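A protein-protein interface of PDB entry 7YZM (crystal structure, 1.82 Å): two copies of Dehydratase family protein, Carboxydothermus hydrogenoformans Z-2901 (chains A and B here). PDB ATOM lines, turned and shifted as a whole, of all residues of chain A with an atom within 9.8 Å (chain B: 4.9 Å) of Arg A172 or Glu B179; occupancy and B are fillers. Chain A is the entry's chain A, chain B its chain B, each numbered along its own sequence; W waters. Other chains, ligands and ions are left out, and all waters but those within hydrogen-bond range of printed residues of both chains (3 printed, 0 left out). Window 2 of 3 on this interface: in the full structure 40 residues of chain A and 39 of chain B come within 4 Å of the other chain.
The side-chain carboxylate (OE2) of Glu B180 lies within salt-bridge range of the guanidinium group (NH1) of Arg A172, 3.3 Å away. NH1 of Arg A172 lies within salt-bridge range of OD2 of Asp B183 (2.7 Å).
NZ of Lys B182 is in salt-bridge range of OE2 of Glu B179, 3.0 Å away. The side-chain carboxylate of Glu B179 is in salt-bridge range of the side-chain amino group of Lys B175, 3.8 Å away. OD2 of Asp A173 is in hydrogen-bond range of N of Glu A170 (3.1 Å).
Among the printed residues, merely in contact across the chains: Arg A172 with Phe B176, Arg A172 with Glu B179, Asp A173 with Phe B176 and Phe A176 with Phe B176.
Leu A165 touches none of the printed residues of chain B. Of the printed residues of chain B, Arg A172 touches Phe B176, Glu B179, Glu B180 and Asp B183. Printed residues of chain B within 4 Å of Asp A173: Phe B176. Of the printed residues of chain B, Phe A176 touches Phe B176 (3.7 Å). Leu A337 touches none of the printed residues of chain B. No residue of chain A comes within 4 Å of Glu B178. Of the printed residues of chain A, Glu B179 touches Arg A172. Of the printed residues of chain A, Glu B180 touches Arg A172 (3.3 Å). No residue of chain A comes within 4 Å of Lys B182. Of the printed residues of chain A, Asp B183 touches Arg A172. The nearest printed residue of chain B that does not touch Asp A173 is Glu B180 (6.0 Å).
Hydrophobic or aromatic side chains of chain B that line the printed part of chain A: Phe B176. Printed residues of chain A that touch a printed residue of chain B: Arg A172, Asp A173 and Phe A176. Among the printed residues, Asp or Glu carboxylates within 4 Å of a Lys or Arg side-chain nitrogen of the other chain: Arg A172 with Glu B180 (3.3 Å) and Arg A172 with Asp B183 (2.7 Å).
Phe A176 touches its own counterpart, Phe B176. Of the 6 pairs that touch across the chains among the printed residues, 1 has its exchanged pair printed and touching as well.
Water W1 lies within hydrogen-bond range of the side-chain carboxylate of Asp B183, the side-chain carboxylate of Glu B179 and the guanidinium group of Arg A172. Water W3 lies within hydrogen-bond range of the side-chain amino group of Lys A168 (2.7 Å) and the side-chain carboxylate of Glu B180 (2.9 Å). Water W2 bridges OD2 of Asp A173 (3.0 Å) and OE2 of Glu B180 (3.2 Å).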
ATOM      1  N   GLU A 164      11.282 -20.064 -18.104  1.00  0.00           N
ATOM      2  CA  GLU A 164      11.971 -20.764 -17.022  1.00  0.00           C
ATOM      3  C   GLU A 164      12.154 -19.813 -15.841  1.00  0.00           C
ATOM      4  O   GLU A 164      13.036 -18.954 -15.848  1.00  0.00           O
ATOM      5  CB  GLU A 164      13.317 -21.335 -17.458  1.00  0.00           C
ATOM      6  CG  GLU A 164      13.942 -22.117 -16.291  1.00  0.00           C
ATOM      7  CD  GLU A 164      15.210 -22.872 -16.615  1.00  0.00           C
ATOM      8  OE1 GLU A 164      15.682 -22.795 -17.768  1.00  0.00           O
ATOM      9  OE2 GLU A 164      15.734 -23.542 -15.688  1.00  0.00           O
ATOM     10  N   LEU A 165      11.331 -19.987 -14.816  1.00  0.00           N
ATOM     11  CA  LEU A 165      11.516 -19.285 -13.553  1.00  0.00           C
ATOM     12  C   LEU A 165      12.594 -19.987 -12.733  1.00  0.00           C
ATOM     13  O   LEU A 165      12.588 -21.219 -12.639  1.00  0.00           O
ATOM     14  CB  LEU A 165      10.200 -19.264 -12.780  1.00  0.00           C
ATOM     15  CG  LEU A 165      10.006 -18.293 -11.628  1.00  0.00           C
ATOM     16  CD1 LEU A 165       9.995 -16.868 -12.135  1.00  0.00           C
ATOM     17  CD2 LEU A 165       8.705 -18.635 -10.909  1.00  0.00           C
ATOM     18  N   PRO A 166      13.533 -19.249 -12.134  1.00  0.00           N
ATOM     19  CA  PRO A 166      14.489 -19.900 -11.227  1.00  0.00           C
ATOM     20  C   PRO A 166      13.807 -20.334  -9.938  1.00  0.00           C
ATOM     21  O   PRO A 166      12.604 -20.102  -9.751  1.00  0.00           O
ATOM     22  CB  PRO A 166      15.548 -18.817 -10.985  1.00  0.00           C
ATOM     23  CG  PRO A 166      14.811 -17.524 -11.171  1.00  0.00           C
ATOM     24  CD  PRO A 166      13.686 -17.783 -12.154  1.00  0.00           C
ATOM     25  N   GLN A 167      14.567 -20.967  -9.046  1.00  0.00           N
ATOM     26  CA  GLN A 167      14.030 -21.510  -7.803  1.00  0.00           C
ATOM     27  C   GLN A 167      14.639 -20.852  -6.573  1.00  0.00           C
ATOM     28  O   GLN A 167      14.244 -21.187  -5.450  1.00  0.00           O
ATOM     29  CB  GLN A 167      14.244 -23.027  -7.775  1.00  0.00           C
ATOM     30  CG  GLN A 167      13.657 -23.683  -9.033  1.00  0.00           C
ATOM     31  CD  GLN A 167      13.702 -25.190  -9.020  1.00  0.00           C
ATOM     32  OE1 GLN A 167      12.942 -25.838  -8.309  1.00  0.00           O
ATOM     33  NE2 GLN A 167      14.575 -25.761  -9.844  1.00  0.00           N
ATOM     34  N   LYS A 168      15.565 -19.912  -6.759  1.00  0.00           N
ATOM     35  CA  LYS A 168      16.081 -19.057  -5.701  1.00  0.00           C
ATOM     36  C   LYS A 168      16.068 -17.614  -6.191  1.00  0.00           C
ATOM     37  O   LYS A 168      15.781 -17.340  -7.358  1.00  0.00           O
ATOM     38  CB  LYS A 168      17.503 -19.459  -5.295  1.00  0.00           C
ATOM     39  CG  LYS A 168      17.601 -20.813  -4.626  1.00  0.00           C
ATOM     40  CD  LYS A 168      19.031 -21.051  -4.172  1.00  0.00           C
ATOM     41  CE  LYS A 168      19.207 -22.429  -3.597  1.00  0.00           C
ATOM     42  NZ  LYS A 168      20.652 -22.716  -3.393  1.00  0.00           N
ATOM     43  N   LYS A 169      16.395 -16.680  -5.294  1.00  0.00           N
ATOM     44  CA  LYS A 169      16.374 -15.262  -5.637  1.00  0.00           C
ATOM     45  C   LYS A 169      17.714 -14.577  -5.399  1.00  0.00           C
ATOM     46  O   LYS A 169      17.767 -13.370  -5.140  1.00  0.00           O
ATOM     47  CB  LYS A 169      15.262 -14.554  -4.873  1.00  0.00           C
ATOM     48  CG  LYS A 169      13.888 -15.091  -5.239  1.00  0.00           C
ATOM     49  CD  LYS A 169      12.797 -14.182  -4.766  1.00  0.00           C
ATOM     50  CE  LYS A 169      11.442 -14.701  -5.175  1.00  0.00           C
ATOM     51  NZ  LYS A 169      10.422 -13.922  -4.430  1.00  0.00           N
ATOM     52  N   GLU A 170      18.798 -15.330  -5.524  1.00  0.00           N
ATOM     53  CA  GLU A 170      20.136 -14.758  -5.493  1.00  0.00           C
ATOM     54  C   GLU A 170      20.408 -13.984  -6.782  1.00  0.00           C
ATOM     55  O   GLU A 170      19.626 -14.014  -7.734  1.00  0.00           O
ATOM     56  CB  GLU A 170      21.185 -15.858  -5.320  1.00  0.00           C
ATOM     57  CG  GLU A 170      20.978 -16.751  -4.111  1.00  0.00           C
ATOM     58  CD  GLU A 170      21.375 -16.077  -2.820  1.00  0.00           C
ATOM     59  OE1 GLU A 170      21.425 -14.828  -2.781  1.00  0.00           O
ATOM     60  OE2 GLU A 170      21.642 -16.799  -1.838  1.00  0.00           O
ATOM     61  N   GLU A 171      21.567 -13.315  -6.816  1.00  0.00           N
ATOM     62  CA  GLU A 171      21.908 -12.463  -7.954  1.00  0.00           C
ATOM     63  C   GLU A 171      21.922 -13.246  -9.261  1.00  0.00           C
ATOM     64  O   GLU A 171      21.418 -12.769 -10.286  1.00  0.00           O
ATOM     65  CB  GLU A 171      23.269 -11.804  -7.716  1.00  0.00           C
ATOM     66  CG  GLU A 171      23.847 -11.121  -8.939  1.00  0.00           C
ATOM     67  CD  GLU A 171      23.072  -9.880  -9.327  1.00  0.00           C
ATOM     68  OE1 GLU A 171      23.407  -9.267 -10.362  1.00  0.00           O
ATOM     69  OE2 GLU A 171      22.124  -9.517  -8.600  1.00  0.00           O
ATOM     70  N   ARG A 172      22.530 -14.431  -9.255  1.00  0.00           N
ATOM     71  CA  ARG A 172      22.539 -15.273 -10.446  1.00  0.00           C
ATOM     72  C   ARG A 172      21.123 -15.545 -10.936  1.00  0.00           C
ATOM     73  O   ARG A 172      20.863 -15.564 -12.142  1.00  0.00           O
ATOM     74  CB  ARG A 172      23.267 -16.577 -10.124  1.00  0.00           C
ATOM     75  CG  ARG A 172      23.653 -17.437 -11.305  1.00  0.00           C
ATOM     76  CD  ARG A 172      24.499 -18.622 -10.834  1.00  0.00           C
ATOM     77  NE  ARG A 172      25.775 -18.193 -10.261  1.00  0.00           N
ATOM     78  CZ  ARG A 172      26.363 -18.763  -9.211  1.00  0.00           C
ATOM     79  NH1 ARG A 172      25.799 -19.799  -8.602  1.00  0.00           N
ATOM     80  NH2 ARG A 172      27.523 -18.296  -8.770  1.00  0.00           N
ATOM     81  N   ASP A 173      20.189 -15.755 -10.004  1.00  0.00           N
ATOM     82  CA  ASP A 173      18.805 -16.024 -10.382  1.00  0.00           C
ATOM     83  C   ASP A 173      18.141 -14.785 -10.959  1.00  0.00           C
ATOM     84  O   ASP A 173      17.379 -14.873 -11.931  1.00  0.00           O
ATOM     85  CB  ASP A 173      18.013 -16.510  -9.168  1.00  0.00           C
ATOM     86  CG  ASP A 173      18.595 -17.764  -8.558  1.00  0.00           C
ATOM     87  OD1 ASP A 173      18.429 -18.839  -9.158  1.00  0.00           O
ATOM     88  OD2 ASP A 173      19.217 -17.677  -7.481  1.00  0.00           O
ATOM     89  N   ARG A 174      18.392 -13.624 -10.353  1.00  0.00           N
ATOM     90  CA  ARG A 174      17.789 -12.394 -10.848  1.00  0.00           C
ATOM     91  C   ARG A 174      18.244 -12.098 -12.270  1.00  0.00           C
ATOM     92  O   ARG A 174      17.435 -11.700 -13.117  1.00  0.00           O
ATOM     93  CB  ARG A 174      18.122 -11.237  -9.905  1.00  0.00           C
ATOM     94  CG  ARG A 174      17.612 -11.493  -8.501  1.00  0.00           C
ATOM     95  CD  ARG A 174      17.779 -10.319  -7.562  1.00  0.00           C
ATOM     96  NE  ARG A 174      17.101 -10.594  -6.298  1.00  0.00           N
ATOM     97  CZ  ARG A 174      15.826 -10.307  -6.050  1.00  0.00           C
ATOM     98  NH1 ARG A 174      15.080  -9.719  -6.975  1.00  0.00           N
ATOM     99  NH2 ARG A 174      15.296 -10.602  -4.872  1.00  0.00           N
ATOM    100  N   LYS A 175      19.531 -12.308 -12.559  1.00  0.00           N
ATOM    101  CA  LYS A 175      20.030 -12.106 -13.915  1.00  0.00           C
ATOM    102  C   LYS A 175      19.436 -13.126 -14.879  1.00  0.00           C
ATOM    103  O   LYS A 175      19.104 -12.792 -16.021  1.00  0.00           O
ATOM    104  CB  LYS A 175      21.555 -12.200 -13.935  1.00  0.00           C
ATOM    105  CG  LYS A 175      22.140 -12.193 -15.337  1.00  0.00           C
ATOM    106  CD  LYS A 175      21.933 -10.841 -16.006  1.00  0.00           C
ATOM    107  CE  LYS A 175      22.889 -10.638 -17.175  1.00  0.00           C
ATOM    108  NZ  LYS A 175      22.445 -11.390 -18.381  1.00  0.00           N
ATOM    109  N   PHE A 176      19.320 -14.380 -14.437  1.00  0.00           N
ATOM    110  CA  PHE A 176      18.710 -15.424 -15.255  1.00  0.00           C
ATOM    111  C   PHE A 176      17.285 -15.039 -15.649  1.00  0.00           C
ATOM    112  O   PHE A 176      16.898 -15.145 -16.817  1.00  0.00           O
ATOM    113  CB  PHE A 176      18.742 -16.749 -14.477  1.00  0.00           C
ATOM    114  CG  PHE A 176      18.339 -17.958 -15.283  1.00  0.00           C
ATOM    115  CD1 PHE A 176      17.008 -18.213 -15.553  1.00  0.00           C
ATOM    116  CD2 PHE A 176      19.293 -18.849 -15.751  1.00  0.00           C
ATOM    117  CE1 PHE A 176      16.635 -19.320 -16.296  1.00  0.00           C
ATOM    118  CE2 PHE A 176      18.922 -19.963 -16.486  1.00  0.00           C
ATOM    119  CZ  PHE A 176      17.593 -20.195 -16.761  1.00  0.00           C
ATOM    120  N   TRP A 177      16.492 -14.576 -14.677  1.00  0.00           N
ATOM    121  CA  TRP A 177      15.116 -14.177 -14.952  1.00  0.00           C
ATOM    122  C   TRP A 177      15.063 -12.954 -15.869  1.00  0.00           C
ATOM    123  O   TRP A 177      14.208 -12.882 -16.763  1.00  0.00           O
ATOM    124  CB  TRP A 177      14.395 -13.925 -13.623  1.00  0.00           C
ATOM    125  CG  TRP A 177      12.943 -13.626 -13.744  1.00  0.00           C
ATOM    126  CD1 TRP A 177      12.301 -12.518 -13.280  1.00  0.00           C
ATOM    127  CD2 TRP A 177      11.938 -14.444 -14.358  1.00  0.00           C
ATOM    128  NE1 TRP A 177      10.964 -12.590 -13.570  1.00  0.00           N
ATOM    129  CE2 TRP A 177      10.718 -13.758 -14.238  1.00  0.00           C
ATOM    130  CE3 TRP A 177      11.956 -15.682 -15.005  1.00  0.00           C
ATOM    131  CZ2 TRP A 177       9.523 -14.271 -14.737  1.00  0.00           C
ATOM    132  CZ3 TRP A 177      10.766 -16.188 -15.501  1.00  0.00           C
ATOM    133  CH2 TRP A 177       9.569 -15.485 -15.360  1.00  0.00           C
ATOM    134  N   GLU A 178      15.985 -12.003 -15.696  1.00  0.00           N
ATOM    135  CA  GLU A 178      16.023 -10.865 -16.614  1.00  0.00           C
ATOM    136  C   GLU A 178      16.166 -11.342 -18.054  1.00  0.00           C
ATOM    137  O   GLU A 178      15.508 -10.822 -18.959  1.00  0.00           O
ATOM    138  CB  GLU A 178      17.175  -9.914 -16.267  1.00  0.00           C
ATOM    139  CG  GLU A 178      16.935  -9.013 -15.065  1.00  0.00           C
ATOM    140  CD  GLU A 178      18.075  -8.017 -14.810  1.00  0.00           C
ATOM    141  OE1 GLU A 178      18.890  -7.760 -15.725  1.00  0.00           O
ATOM    142  OE2 GLU A 178      18.146  -7.484 -13.683  1.00  0.00           O
ATOM    143  N   GLU A 179      17.021 -12.343 -18.280  1.00  0.00           N
ATOM    144  CA  GLU A 179      17.207 -12.866 -19.628  1.00  0.00           C
ATOM    145  C   GLU A 179      15.956 -13.586 -20.122  1.00  0.00           C
ATOM    146  O   GLU A 179      15.615 -13.502 -21.306  1.00  0.00           O
ATOM    147  CB  GLU A 179      18.417 -13.802 -19.665  1.00  0.00           C
ATOM    148  CG  GLU A 179      19.754 -13.122 -19.383  1.00  0.00           C
ATOM    149  CD  GLU A 179      20.014 -11.937 -20.296  1.00  0.00           C
ATOM    150  OE1 GLU A 179      19.863 -12.083 -21.527  1.00  0.00           O
ATOM    151  OE2 GLU A 179      20.362 -10.852 -19.780  1.00  0.00           O
ATOM    152  N   GLU A 180      15.261 -14.305 -19.239  1.00  0.00           N
ATOM    153  CA  GLU A 180      14.027 -14.973 -19.647  1.00  0.00           C
ATOM    154  C   GLU A 180      12.963 -13.959 -20.046  1.00  0.00           C
ATOM    155  O   GLU A 180      12.171 -14.200 -20.969  1.00  0.00           O
ATOM    156  CB  GLU A 180      13.507 -15.856 -18.514  1.00  0.00           C
ATOM    157  CG  GLU A 180      14.316 -17.117 -18.304  1.00  0.00           C
ATOM    158  CD  GLU A 180      14.123 -18.153 -19.400  1.00  0.00           C
ATOM    159  OE1 GLU A 180      12.966 -18.402 -19.818  1.00  0.00           O
ATOM    160  OE2 GLU A 180      15.139 -18.734 -19.832  1.00  0.00           O
ATOM    161  N   LEU A 337       9.647 -10.847  -9.478  1.00  0.00           N
ATOM    162  CA  LEU A 337      10.459 -11.579  -8.513  1.00  0.00           C
ATOM    163  C   LEU A 337      10.205 -11.145  -7.080  1.00  0.00           C
ATOM    164  O   LEU A 337      10.698 -11.800  -6.155  1.00  0.00           O
ATOM    165  CB  LEU A 337      11.946 -11.414  -8.829  1.00  0.00           C
ATOM    166  CG  LEU A 337      12.522 -12.389  -9.853  1.00  0.00           C
ATOM    167  CD1 LEU A 337      14.018 -12.163 -10.032  1.00  0.00           C
ATOM    168  CD2 LEU A 337      12.256 -13.839  -9.463  1.00  0.00           C
ATOM    169  N   LYS B 175      25.438 -23.096 -18.386  1.00  0.00           N
ATOM    170  CA  LYS B 175      26.332 -22.153 -17.720  1.00  0.00           C
ATOM    171  C   LYS B 175      25.938 -21.983 -16.256  1.00  0.00           C
ATOM    172  O   LYS B 175      26.788 -22.025 -15.363  1.00  0.00           O
ATOM    173  CB  LYS B 175      26.307 -20.813 -18.456  1.00  0.00           C
ATOM    174  CG  LYS B 175      27.107 -19.720 -17.777  1.00  0.00           C
ATOM    175  CD  LYS B 175      28.586 -20.077 -17.719  1.00  0.00           C
ATOM    176  CE  LYS B 175      29.428 -18.908 -17.224  1.00  0.00           C
ATOM    177  NZ  LYS B 175      30.862 -19.051 -17.610  1.00  0.00           N
ATOM    178  N   PHE B 176      24.644 -21.797 -15.998  1.00  0.00           N
ATOM    179  CA  PHE B 176      24.141 -21.704 -14.633  1.00  0.00           C
ATOM    180  C   PHE B 176      24.599 -22.884 -13.782  1.00  0.00           C
ATOM    181  O   PHE B 176      25.078 -22.707 -12.654  1.00  0.00           O
ATOM    182  CB  PHE B 176      22.616 -21.622 -14.684  1.00  0.00           C
ATOM    183  CG  PHE B 176      21.974 -21.278 -13.381  1.00  0.00           C
ATOM    184  CD1 PHE B 176      21.693 -22.265 -12.454  1.00  0.00           C
ATOM    185  CD2 PHE B 176      21.628 -19.972 -13.089  1.00  0.00           C
ATOM    186  CE1 PHE B 176      21.095 -21.955 -11.253  1.00  0.00           C
ATOM    187  CE2 PHE B 176      21.017 -19.657 -11.887  1.00  0.00           C
ATOM    188  CZ  PHE B 176      20.753 -20.650 -10.970  1.00  0.00           C
ATOM    189  N   TRP B 177      24.453 -24.104 -14.303  1.00  0.00           N
ATOM    190  CA  TRP B 177      24.802 -25.285 -13.522  1.00  0.00           C
ATOM    191  C   TRP B 177      26.307 -25.374 -13.296  1.00  0.00           C
ATOM    192  O   TRP B 177      26.757 -25.815 -12.230  1.00  0.00           O
ATOM    193  CB  TRP B 177      24.298 -26.538 -14.233  1.00  0.00           C
ATOM    194  CG  TRP B 177      24.567 -27.837 -13.521  1.00  0.00           C
ATOM    195  CD1 TRP B 177      25.213 -28.921 -14.033  1.00  0.00           C
ATOM    196  CD2 TRP B 177      24.179 -28.194 -12.186  1.00  0.00           C
ATOM    197  NE1 TRP B 177      25.255 -29.929 -13.104  1.00  0.00           N
ATOM    198  CE2 TRP B 177      24.629 -29.510 -11.962  1.00  0.00           C
ATOM    199  CE3 TRP B 177      23.498 -27.531 -11.160  1.00  0.00           C
ATOM    200  CZ2 TRP B 177      24.416 -30.178 -10.758  1.00  0.00           C
ATOM    201  CZ3 TRP B 177      23.292 -28.194  -9.966  1.00  0.00           C
ATOM    202  CH2 TRP B 177      23.753 -29.502  -9.772  1.00  0.00           C
ATOM    203  N   GLU B 178      27.095 -24.986 -14.296  1.00  0.00           N
ATOM    204  CA  GLU B 178      28.538 -24.896 -14.107  1.00  0.00           C
ATOM    205  C   GLU B 178      28.874 -23.982 -12.934  1.00  0.00           C
ATOM    206  O   GLU B 178      29.756 -24.293 -12.126  1.00  0.00           O
ATOM    207  CB  GLU B 178      29.177 -24.402 -15.404  1.00  0.00           C
ATOM    208  CG  GLU B 178      30.655 -24.114 -15.349  1.00  0.00           C
ATOM    209  CD  GLU B 178      31.172 -23.627 -16.691  1.00  0.00           C
ATOM    210  OE1 GLU B 178      30.707 -24.149 -17.731  1.00  0.00           O
ATOM    211  OE2 GLU B 178      32.026 -22.713 -16.704  1.00  0.00           O
ATOM    212  N   GLU B 179      28.154 -22.868 -12.802  1.00  0.00           N
ATOM    213  CA  GLU B 179      28.408 -21.958 -11.690  1.00  0.00           C
ATOM    214  C   GLU B 179      27.980 -22.572 -10.361  1.00  0.00           C
ATOM    215  O   GLU B 179      28.635 -22.357  -9.336  1.00  0.00           O
ATOM    216  CB  GLU B 179      27.696 -20.631 -11.935  1.00  0.00           C
ATOM    217  CG  GLU B 179      28.231 -19.857 -13.132  1.00  0.00           C
ATOM    218  CD  GLU B 179      29.705 -19.525 -12.990  1.00  0.00           C
ATOM    219  OE1 GLU B 179      30.095 -18.970 -11.934  1.00  0.00           O
ATOM    220  OE2 GLU B 179      30.475 -19.834 -13.929  1.00  0.00           O
ATOM    221  N   GLU B 180      26.881 -23.332 -10.351  1.00  0.00           N
ATOM    222  CA  GLU B 180      26.486 -24.036  -9.135  1.00  0.00           C
ATOM    223  C   GLU B 180      27.552 -25.032  -8.703  1.00  0.00           C
ATOM    224  O   GLU B 180      27.826 -25.187  -7.504  1.00  0.00           O
ATOM    225  CB  GLU B 180      25.159 -24.764  -9.356  1.00  0.00           C
ATOM    226  CG  GLU B 180      23.959 -23.853  -9.389  1.00  0.00           C
ATOM    227  CD  GLU B 180      23.644 -23.250  -8.038  1.00  0.00           C
ATOM    228  OE1 GLU B 180      23.643 -23.988  -7.026  1.00  0.00           O
ATOM    229  OE2 GLU B 180      23.394 -22.028  -7.994  1.00  0.00           O
ATOM    230  N   ILE B 181      28.141 -25.742  -9.667  1.00  0.00           N
ATOM    231  CA  ILE B 181      29.173 -26.724  -9.349  1.00  0.00           C
ATOM    232  C   ILE B 181      30.411 -26.027  -8.793  1.00  0.00           C
ATOM    233  O   ILE B 181      31.069 -26.532  -7.874  1.00  0.00           O
ATOM    234  CB  ILE B 181      29.494 -27.570 -10.597  1.00  0.00           C
ATOM    235  CG1 ILE B 181      28.298 -28.464 -10.947  1.00  0.00           C
ATOM    236  CG2 ILE B 181      30.779 -28.374 -10.394  1.00  0.00           C
ATOM    237  CD1 ILE B 181      28.098 -29.643 -10.018  1.00  0.00           C
ATOM    238  N   LYS B 182      30.739 -24.852  -9.330  1.00  0.00           N
ATOM    239  CA  LYS B 182      31.865 -24.081  -8.816  1.00  0.00           C
ATOM    240  C   LYS B 182      31.599 -23.585  -7.399  1.00  0.00           C
ATOM    241  O   LYS B 182      32.500 -23.600  -6.553  1.00  0.00           O
ATOM    242  CB  LYS B 182      32.157 -22.909  -9.754  1.00  0.00           C
ATOM    243  CG  LYS B 182      32.994 -23.299 -10.960  1.00  0.00           C
ATOM    244  CD  LYS B 182      32.761 -22.374 -12.143  1.00  0.00           C
ATOM    245  CE  LYS B 182      33.253 -20.965 -11.859  1.00  0.00           C
ATOM    246  NZ  LYS B 182      33.381 -20.169 -13.111  1.00  0.00           N
ATOM    247  N   ASP B 183      30.371 -23.139  -7.120  1.00  0.00           N
ATOM    248  CA  ASP B 183      30.022 -22.748  -5.759  1.00  0.00           C
ATOM    249  C   ASP B 183      30.062 -23.939  -4.817  1.00  0.00           C
ATOM    250  O   ASP B 183      30.522 -23.826  -3.676  1.00  0.00           O
ATOM    251  CB  ASP B 183      28.632 -22.116  -5.724  1.00  0.00           C
ATOM    252  CG  ASP B 183      28.599 -20.756  -6.375  1.00  0.00           C
ATOM    253  OD1 ASP B 183      29.673 -20.267  -6.776  1.00  0.00           O
ATOM    254  OD2 ASP B 183      27.497 -20.184  -6.492  1.00  0.00           O
HETATM  255  O   HOH W   1      30.234 -19.684  -9.097  1.00  0.00           O
HETATM  256  O   HOH W   2      21.521 -19.617  -7.039  1.00  0.00           O
HETATM  257  O   HOH W   3      22.324 -21.847  -5.264  1.00  0.00           O
